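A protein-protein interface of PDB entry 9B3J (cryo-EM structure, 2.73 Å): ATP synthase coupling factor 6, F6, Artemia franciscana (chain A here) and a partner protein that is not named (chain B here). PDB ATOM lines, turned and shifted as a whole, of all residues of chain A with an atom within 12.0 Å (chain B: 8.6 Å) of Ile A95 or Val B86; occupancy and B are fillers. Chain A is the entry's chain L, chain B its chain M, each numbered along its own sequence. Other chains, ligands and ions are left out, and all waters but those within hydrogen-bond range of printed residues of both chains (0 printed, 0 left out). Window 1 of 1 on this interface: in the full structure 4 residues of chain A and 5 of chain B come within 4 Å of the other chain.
OD1 of Asp A93 sits close to OH of Tyr B38, at 3.2 Å.
ND2 of Asn A96 sits at hydrogen-bond distance from OE1 of Gln B93, at 2.6 Å.
OD1 of Asp B84 lies within hydrogen-bond range of N of Val B86 (2.8 Å).
Among the printed residues, merely in contact across the chains: Ile A95 with Val B86 (3.9 Å) and Ile A95 with Gln B93 (3.6 Å).
Of the printed residues of chain B, Ile A95 touches Val B86 (3.9 Å) and Gln B93 (3.6 Å).
Of the printed residues of chain B, Asn A96 touches Gln B93 (2.6 Å).
Met B27 touches none of the printed residues of chain A.
Lys B34 touches none of the printed residues of chain A.
Of the printed residues of chain A, Tyr B38 touches Asp A93 (3.1 Å).
No residue of chain A comes within 4 Å of Ser B87.
No residue of chain A comes within 4 Å of Ser B88.
No residue of chain A comes within 4 Å of Gln B89.
No residue of chain A comes within 4 Å of Ile B90.
Of the printed residues of chain A, Gln B93 touches Ile A95 and Asn A96.
The nearest residue of chain A that does not touch Val B86 is Val A92 (4.6 Å).
The nearest printed residue of chain B that does not touch Asp A93 is Lys B34 (4.9 Å).
Hydrophobic or aromatic side chains of chain A within 4 Å of the printed part of chain B: Ile A95.
Of the 15 printed residues of chain B, 3 touch a printed residue of chain A.
Hydrophobic or aromatic side chains of chain B that line the printed part of chain A: Tyr B38 and Val B86.
Among the printed residues, no Asp or Glu carboxylate lies within 4 Å of a Lys or Arg side-chain nitrogen of the other chain.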
ATOM      1  N   ASP A  89      18.343  34.286  32.702  1.00  0.00           N
ATOM      2  CA  ASP A  89      18.803  33.156  31.908  1.00  0.00           C
ATOM      3  C   ASP A  89      17.690  32.589  31.036  1.00  0.00           C
ATOM      4  O   ASP A  89      16.638  32.198  31.562  1.00  0.00           O
ATOM      5  CB  ASP A  89      19.377  32.079  32.812  1.00  0.00           C
ATOM      6  CG  ASP A  89      20.844  32.294  33.090  1.00  0.00           C
ATOM      7  OD1 ASP A  89      21.191  33.384  33.582  1.00  0.00           O
ATOM      8  OD2 ASP A  89      21.651  31.387  32.800  1.00  0.00           O
ATOM      9  N   PRO A  90      17.872  32.539  29.714  1.00  0.00           N
ATOM     10  CA  PRO A  90      16.748  32.265  28.814  1.00  0.00           C
ATOM     11  C   PRO A  90      16.503  30.783  28.592  1.00  0.00           C
ATOM     12  O   PRO A  90      17.425  29.973  28.481  1.00  0.00           O
ATOM     13  CB  PRO A  90      17.192  32.947  27.513  1.00  0.00           C
ATOM     14  CG  PRO A  90      18.680  32.838  27.535  1.00  0.00           C
ATOM     15  CD  PRO A  90      19.108  32.869  28.973  1.00  0.00           C
ATOM     16  N   VAL A  91      15.222  30.434  28.539  1.00  0.00           N
ATOM     17  CA  VAL A  91      14.774  29.090  28.205  1.00  0.00           C
ATOM     18  C   VAL A  91      13.978  29.204  26.916  1.00  0.00           C
ATOM     19  O   VAL A  91      12.895  29.803  26.900  1.00  0.00           O
ATOM     20  CB  VAL A  91      13.932  28.463  29.323  1.00  0.00           C
ATOM     21  CG1 VAL A  91      13.396  27.110  28.883  1.00  0.00           C
ATOM     22  CG2 VAL A  91      14.753  28.329  30.597  1.00  0.00           C
ATOM     23  N   VAL A  92      14.508  28.635  25.839  1.00  0.00           N
ATOM     24  CA  VAL A  92      13.862  28.727  24.537  1.00  0.00           C
ATOM     25  C   VAL A  92      12.699  27.749  24.477  1.00  0.00           C
ATOM     26  O   VAL A  92      12.556  26.879  25.345  1.00  0.00           O
ATOM     27  CB  VAL A  92      14.862  28.464  23.398  1.00  0.00           C
ATOM     28  CG1 VAL A  92      16.010  29.450  23.477  1.00  0.00           C
ATOM     29  CG2 VAL A  92      15.370  27.034  23.460  1.00  0.00           C
ATOM     30  N   ASP A  93      11.856  27.900  23.460  1.00  0.00           N
ATOM     31  CA  ASP A  93      10.759  26.975  23.249  1.00  0.00           C
ATOM     32  C   ASP A  93      11.301  25.593  22.885  1.00  0.00           C
ATOM     33  O   ASP A  93      12.391  25.479  22.317  1.00  0.00           O
ATOM     34  CB  ASP A  93       9.845  27.485  22.137  1.00  0.00           C
ATOM     35  CG  ASP A  93      10.559  27.596  20.806  1.00  0.00           C
ATOM     36  OD1 ASP A  93      11.758  27.943  20.801  1.00  0.00           O
ATOM     37  OD2 ASP A  93       9.923  27.332  19.764  1.00  0.00           O
ATOM     38  N   PRO A  94      10.572  24.522  23.230  1.00  0.00           N
ATOM     39  CA  PRO A  94      11.032  23.175  22.863  1.00  0.00           C
ATOM     40  C   PRO A  94      11.056  22.962  21.360  1.00  0.00           C
ATOM     41  O   PRO A  94      10.010  22.929  20.704  1.00  0.00           O
ATOM     42  CB  PRO A  94      10.012  22.253  23.547  1.00  0.00           C
ATOM     43  CG  PRO A  94       8.817  23.112  23.791  1.00  0.00           C
ATOM     44  CD  PRO A  94       9.361  24.476  24.068  1.00  0.00           C
ATOM     45  N   ILE A  95      12.267  22.838  20.814  1.00  0.00           N
ATOM     46  CA  ILE A  95      12.432  22.548  19.394  1.00  0.00           C
ATOM     47  C   ILE A  95      11.840  21.185  19.070  1.00  0.00           C
ATOM     48  O   ILE A  95      11.118  21.019  18.078  1.00  0.00           O
ATOM     49  CB  ILE A  95      13.920  22.632  19.003  1.00  0.00           C
ATOM     50  CG1 ILE A  95      14.446  24.061  19.174  1.00  0.00           C
ATOM     51  CG2 ILE A  95      14.138  22.150  17.580  1.00  0.00           C
ATOM     52  CD1 ILE A  95      15.254  24.281  20.440  1.00  0.00           C
ATOM     53  N   ASN A  96      12.110  20.199  19.916  1.00  0.00           N
ATOM     54  CA  ASN A  96      11.521  18.885  19.752  1.00  0.00           C
ATOM     55  C   ASN A  96      10.070  18.889  20.232  1.00  0.00           C
ATOM     56  O   ASN A  96       9.595  19.833  20.870  1.00  0.00           O
ATOM     57  CB  ASN A  96      12.345  17.836  20.492  1.00  0.00           C
ATOM     58  CG  ASN A  96      13.781  17.786  20.010  1.00  0.00           C
ATOM     59  OD1 ASN A  96      14.100  17.098  19.038  1.00  0.00           O
ATOM     60  ND2 ASN A  96      14.654  18.526  20.681  1.00  0.00           N
ATOM     61  N   MET A  97       9.354  17.823  19.884  1.00  0.00           N
ATOM     62  CA  MET A  97       7.946  17.687  20.240  1.00  0.00           C
ATOM     63  C   MET A  97       7.785  16.953  21.564  1.00  0.00           C
ATOM     64  O   MET A  97       8.159  17.466  22.618  1.00  0.00           O
ATOM     65  CB  MET A  97       7.179  16.954  19.135  1.00  0.00           C
ATOM     66  CG  MET A  97       5.707  16.734  19.435  1.00  0.00           C
ATOM     67  SD  MET A  97       4.818  15.998  18.049  1.00  0.00           S
ATOM     68  CE  MET A  97       5.744  14.485  17.813  1.00  0.00           C
ATOM     69  N   MET B  27       2.161  21.218  12.012  1.00  0.00           N
ATOM     70  CA  MET B  27       3.045  21.944  12.915  1.00  0.00           C
ATOM     71  C   MET B  27       3.827  23.039  12.202  1.00  0.00           C
ATOM     72  O   MET B  27       4.337  23.949  12.866  1.00  0.00           O
ATOM     73  CB  MET B  27       4.008  20.973  13.594  1.00  0.00           C
ATOM     74  CG  MET B  27       3.324  19.850  14.353  1.00  0.00           C
ATOM     75  SD  MET B  27       2.320  20.453  15.723  1.00  0.00           S
ATOM     76  CE  MET B  27       1.806  18.909  16.469  1.00  0.00           C
ATOM     77  N   PHE B  31       5.106  26.523  13.155  1.00  0.00           N
ATOM     78  CA  PHE B  31       6.499  26.918  12.972  1.00  0.00           C
ATOM     79  C   PHE B  31       6.607  28.241  12.228  1.00  0.00           C
ATOM     80  O   PHE B  31       7.486  29.057  12.527  1.00  0.00           O
ATOM     81  CB  PHE B  31       7.267  25.827  12.227  1.00  0.00           C
ATOM     82  CG  PHE B  31       8.746  26.071  12.158  1.00  0.00           C
ATOM     83  CD1 PHE B  31       9.560  25.750  13.229  1.00  0.00           C
ATOM     84  CD2 PHE B  31       9.323  26.619  11.024  1.00  0.00           C
ATOM     85  CE1 PHE B  31      10.921  25.973  13.172  1.00  0.00           C
ATOM     86  CE2 PHE B  31      10.686  26.843  10.962  1.00  0.00           C
ATOM     87  CZ  PHE B  31      11.485  26.519  12.036  1.00  0.00           C
ATOM     88  N   LYS B  34       5.092  30.630  15.324  1.00  0.00           N
ATOM     89  CA  LYS B  34       5.877  30.804  16.544  1.00  0.00           C
ATOM     90  C   LYS B  34       7.182  31.534  16.261  1.00  0.00           C
ATOM     91  O   LYS B  34       7.581  32.422  17.026  1.00  0.00           O
ATOM     92  CB  LYS B  34       6.149  29.452  17.196  1.00  0.00           C
ATOM     93  CG  LYS B  34       4.908  28.766  17.724  1.00  0.00           C
ATOM     94  CD  LYS B  34       5.250  27.414  18.317  1.00  0.00           C
ATOM     95  CE  LYS B  34       4.004  26.682  18.774  1.00  0.00           C
ATOM     96  NZ  LYS B  34       4.336  25.349  19.342  1.00  0.00           N
ATOM     97  N   TYR B  38       9.058  35.349  17.295  1.00  0.00           N
ATOM     98  CA  TYR B  38      10.447  35.767  17.412  1.00  0.00           C
ATOM     99  C   TYR B  38      10.840  36.771  16.338  1.00  0.00           C
ATOM    100  O   TYR B  38      11.929  37.349  16.425  1.00  0.00           O
ATOM    101  CB  TYR B  38      11.365  34.549  17.357  1.00  0.00           C
ATOM    102  CG  TYR B  38      11.044  33.517  18.408  1.00  0.00           C
ATOM    103  CD1 TYR B  38      11.181  33.810  19.757  1.00  0.00           C
ATOM    104  CD2 TYR B  38      10.605  32.248  18.053  1.00  0.00           C
ATOM    105  CE1 TYR B  38      10.889  32.870  20.724  1.00  0.00           C
ATOM    106  CE2 TYR B  38      10.310  31.300  19.013  1.00  0.00           C
ATOM    107  CZ  TYR B  38      10.455  31.616  20.347  1.00  0.00           C
ATOM    108  OH  TYR B  38      10.163  30.678  21.309  1.00  0.00           O
ATOM    109  N   GLU B  83      25.181  33.419  25.908  1.00  0.00           N
ATOM    110  CA  GLU B  83      25.752  32.089  25.769  1.00  0.00           C
ATOM    111  C   GLU B  83      24.752  31.143  25.117  1.00  0.00           C
ATOM    112  O   GLU B  83      23.536  31.341  25.186  1.00  0.00           O
ATOM    113  CB  GLU B  83      26.188  31.554  27.130  1.00  0.00           C
ATOM    114  CG  GLU B  83      27.450  32.210  27.678  1.00  0.00           C
ATOM    115  CD  GLU B  83      28.728  31.585  27.138  1.00  0.00           C
ATOM    116  OE1 GLU B  83      28.643  30.556  26.435  1.00  0.00           O
ATOM    117  OE2 GLU B  83      29.820  32.120  27.425  1.00  0.00           O
ATOM    118  N   ASP B  84      25.282  30.115  24.457  1.00  0.00           N
ATOM    119  CA  ASP B  84      24.468  29.133  23.755  1.00  0.00           C
ATOM    120  C   ASP B  84      24.836  27.731  24.213  1.00  0.00           C
ATOM    121  O   ASP B  84      26.017  27.401  24.358  1.00  0.00           O
ATOM    122  CB  ASP B  84      24.643  29.242  22.237  1.00  0.00           C
ATOM    123  CG  ASP B  84      23.722  28.306  21.473  1.00  0.00           C
ATOM    124  OD1 ASP B  84      22.703  27.860  22.043  1.00  0.00           O
ATOM    125  OD2 ASP B  84      24.020  28.014  20.296  1.00  0.00           O
ATOM    126  N   LYS B  85      23.810  26.909  24.435  1.00  0.00           N
ATOM    127  CA  LYS B  85      23.984  25.495  24.739  1.00  0.00           C
ATOM    128  C   LYS B  85      23.058  24.617  23.907  1.00  0.00           C
ATOM    129  O   LYS B  85      23.005  23.403  24.134  1.00  0.00           O
ATOM    130  CB  LYS B  85      23.756  25.223  26.230  1.00  0.00           C
ATOM    131  CG  LYS B  85      24.842  25.770  27.138  1.00  0.00           C
ATOM    132  CD  LYS B  85      24.590  25.400  28.589  1.00  0.00           C
ATOM    133  CE  LYS B  85      25.663  25.973  29.497  1.00  0.00           C
ATOM    134  NZ  LYS B  85      25.444  25.594  30.920  1.00  0.00           N
ATOM    135  N   VAL B  86      22.324  25.199  22.956  1.00  0.00           N
ATOM    136  CA  VAL B  86      21.422  24.443  22.096  1.00  0.00           C
ATOM    137  C   VAL B  86      22.054  24.102  20.755  1.00  0.00           C
ATOM    138  O   VAL B  86      21.431  23.401  19.946  1.00  0.00           O
ATOM    139  CB  VAL B  86      20.098  25.206  21.884  1.00  0.00           C
ATOM    140  CG1 VAL B  86      18.923  24.243  21.837  1.00  0.00           C
ATOM    141  CG2 VAL B  86      19.895  26.242  22.977  1.00  0.00           C
ATOM    142  N   SER B  87      23.275  24.578  20.496  1.00  0.00           N
ATOM    143  CA  SER B  87      23.927  24.317  19.215  1.00  0.00           C
ATOM    144  C   SER B  87      24.252  22.839  19.042  1.00  0.00           C
ATOM    145  O   SER B  87      24.054  22.278  17.957  1.00  0.00           O
ATOM    146  CB  SER B  87      25.197  25.156  19.097  1.00  0.00           C
ATOM    147  OG  SER B  87      26.111  24.833  20.131  1.00  0.00           O
ATOM    148  N   SER B  88      24.754  22.195  20.098  1.00  0.00           N
ATOM    149  CA  SER B  88      25.085  20.776  20.015  1.00  0.00           C
ATOM    150  C   SER B  88      23.833  19.924  19.854  1.00  0.00           C
ATOM    151  O   SER B  88      23.852  18.909  19.149  1.00  0.00           O
ATOM    152  CB  SER B  88      25.868  20.347  21.254  1.00  0.00           C
ATOM    153  OG  SER B  88      25.111  20.560  22.432  1.00  0.00           O
ATOM    154  N   GLN B  89      22.736  20.327  20.500  1.00  0.00           N
ATOM    155  CA  GLN B  89      21.474  19.608  20.357  1.00  0.00           C
ATOM    156  C   GLN B  89      20.938  19.707  18.935  1.00  0.00           C
ATOM    157  O   GLN B  89      20.462  18.713  18.372  1.00  0.00           O
ATOM    158  CB  GLN B  89      20.453  20.157  21.350  1.00  0.00           C
ATOM    159  CG  GLN B  89      21.050  20.489  22.703  1.00  0.00           C
ATOM    160  CD  GLN B  89      20.118  21.315  23.558  1.00  0.00           C
ATOM    161  OE1 GLN B  89      18.901  21.292  23.372  1.00  0.00           O
ATOM    162  NE2 GLN B  89      20.684  22.062  24.498  1.00  0.00           N
ATOM    163  N   ILE B  90      21.018  20.897  18.338  1.00  0.00           N
ATOM    164  CA  ILE B  90      20.549  21.085  16.970  1.00  0.00           C
ATOM    165  C   ILE B  90      21.439  20.330  15.990  1.00  0.00           C
ATOM    166  O   ILE B  90      20.951  19.744  15.018  1.00  0.00           O
ATOM    167  CB  ILE B  90      20.468  22.590  16.653  1.00  0.00           C
ATOM    168  CG1 ILE B  90      19.323  23.223  17.447  1.00  0.00           C
ATOM    169  CG2 ILE B  90      20.279  22.844  15.165  1.00  0.00           C
ATOM    170  CD1 ILE B  90      19.188  24.711  17.247  1.00  0.00           C
ATOM    171  N   ASP B  91      22.750  20.304  16.244  1.00  0.00           N
ATOM    172  CA  ASP B  91      23.656  19.527  15.402  1.00  0.00           C
ATOM    173  C   ASP B  91      23.379  18.032  15.509  1.00  0.00           C
ATOM    174  O   ASP B  91      23.464  17.307  14.510  1.00  0.00           O
ATOM    175  CB  ASP B  91      25.104  19.826  15.775  1.00  0.00           C
ATOM    176  CG  ASP B  91      25.515  21.231  15.411  1.00  0.00           C
ATOM    177  OD1 ASP B  91      24.991  21.759  14.407  1.00  0.00           O
ATOM    178  OD2 ASP B  91      26.356  21.810  16.130  1.00  0.00           O
ATOM    179  N   ALA B  92      23.057  17.551  16.713  1.00  0.00           N
ATOM    180  CA  ALA B  92      22.693  16.147  16.881  1.00  0.00           C
ATOM    181  C   ALA B  92      21.392  15.822  16.157  1.00  0.00           C
ATOM    182  O   ALA B  92      21.276  14.765  15.521  1.00  0.00           O
ATOM    183  CB  ALA B  92      22.580  15.810  18.366  1.00  0.00           C
ATOM    184  N   GLN B  93      20.408  16.722  16.240  1.00  0.00           N
ATOM    185  CA  GLN B  93      19.163  16.535  15.502  1.00  0.00           C
ATOM    186  C   GLN B  93      19.403  16.570  13.999  1.00  0.00           C
ATOM    187  O   GLN B  93      18.776  15.818  13.246  1.00  0.00           O
ATOM    188  CB  GLN B  93      18.148  17.605  15.897  1.00  0.00           C
ATOM    189  CG  GLN B  93      17.640  17.499  17.318  1.00  0.00           C
ATOM    190  CD  GLN B  93      16.808  18.699  17.717  1.00  0.00           C
ATOM    191  OE1 GLN B  93      16.531  18.914  18.898  1.00  0.00           O
ATOM    192  NE2 GLN B  93      16.404  19.493  16.733  1.00  0.00           N
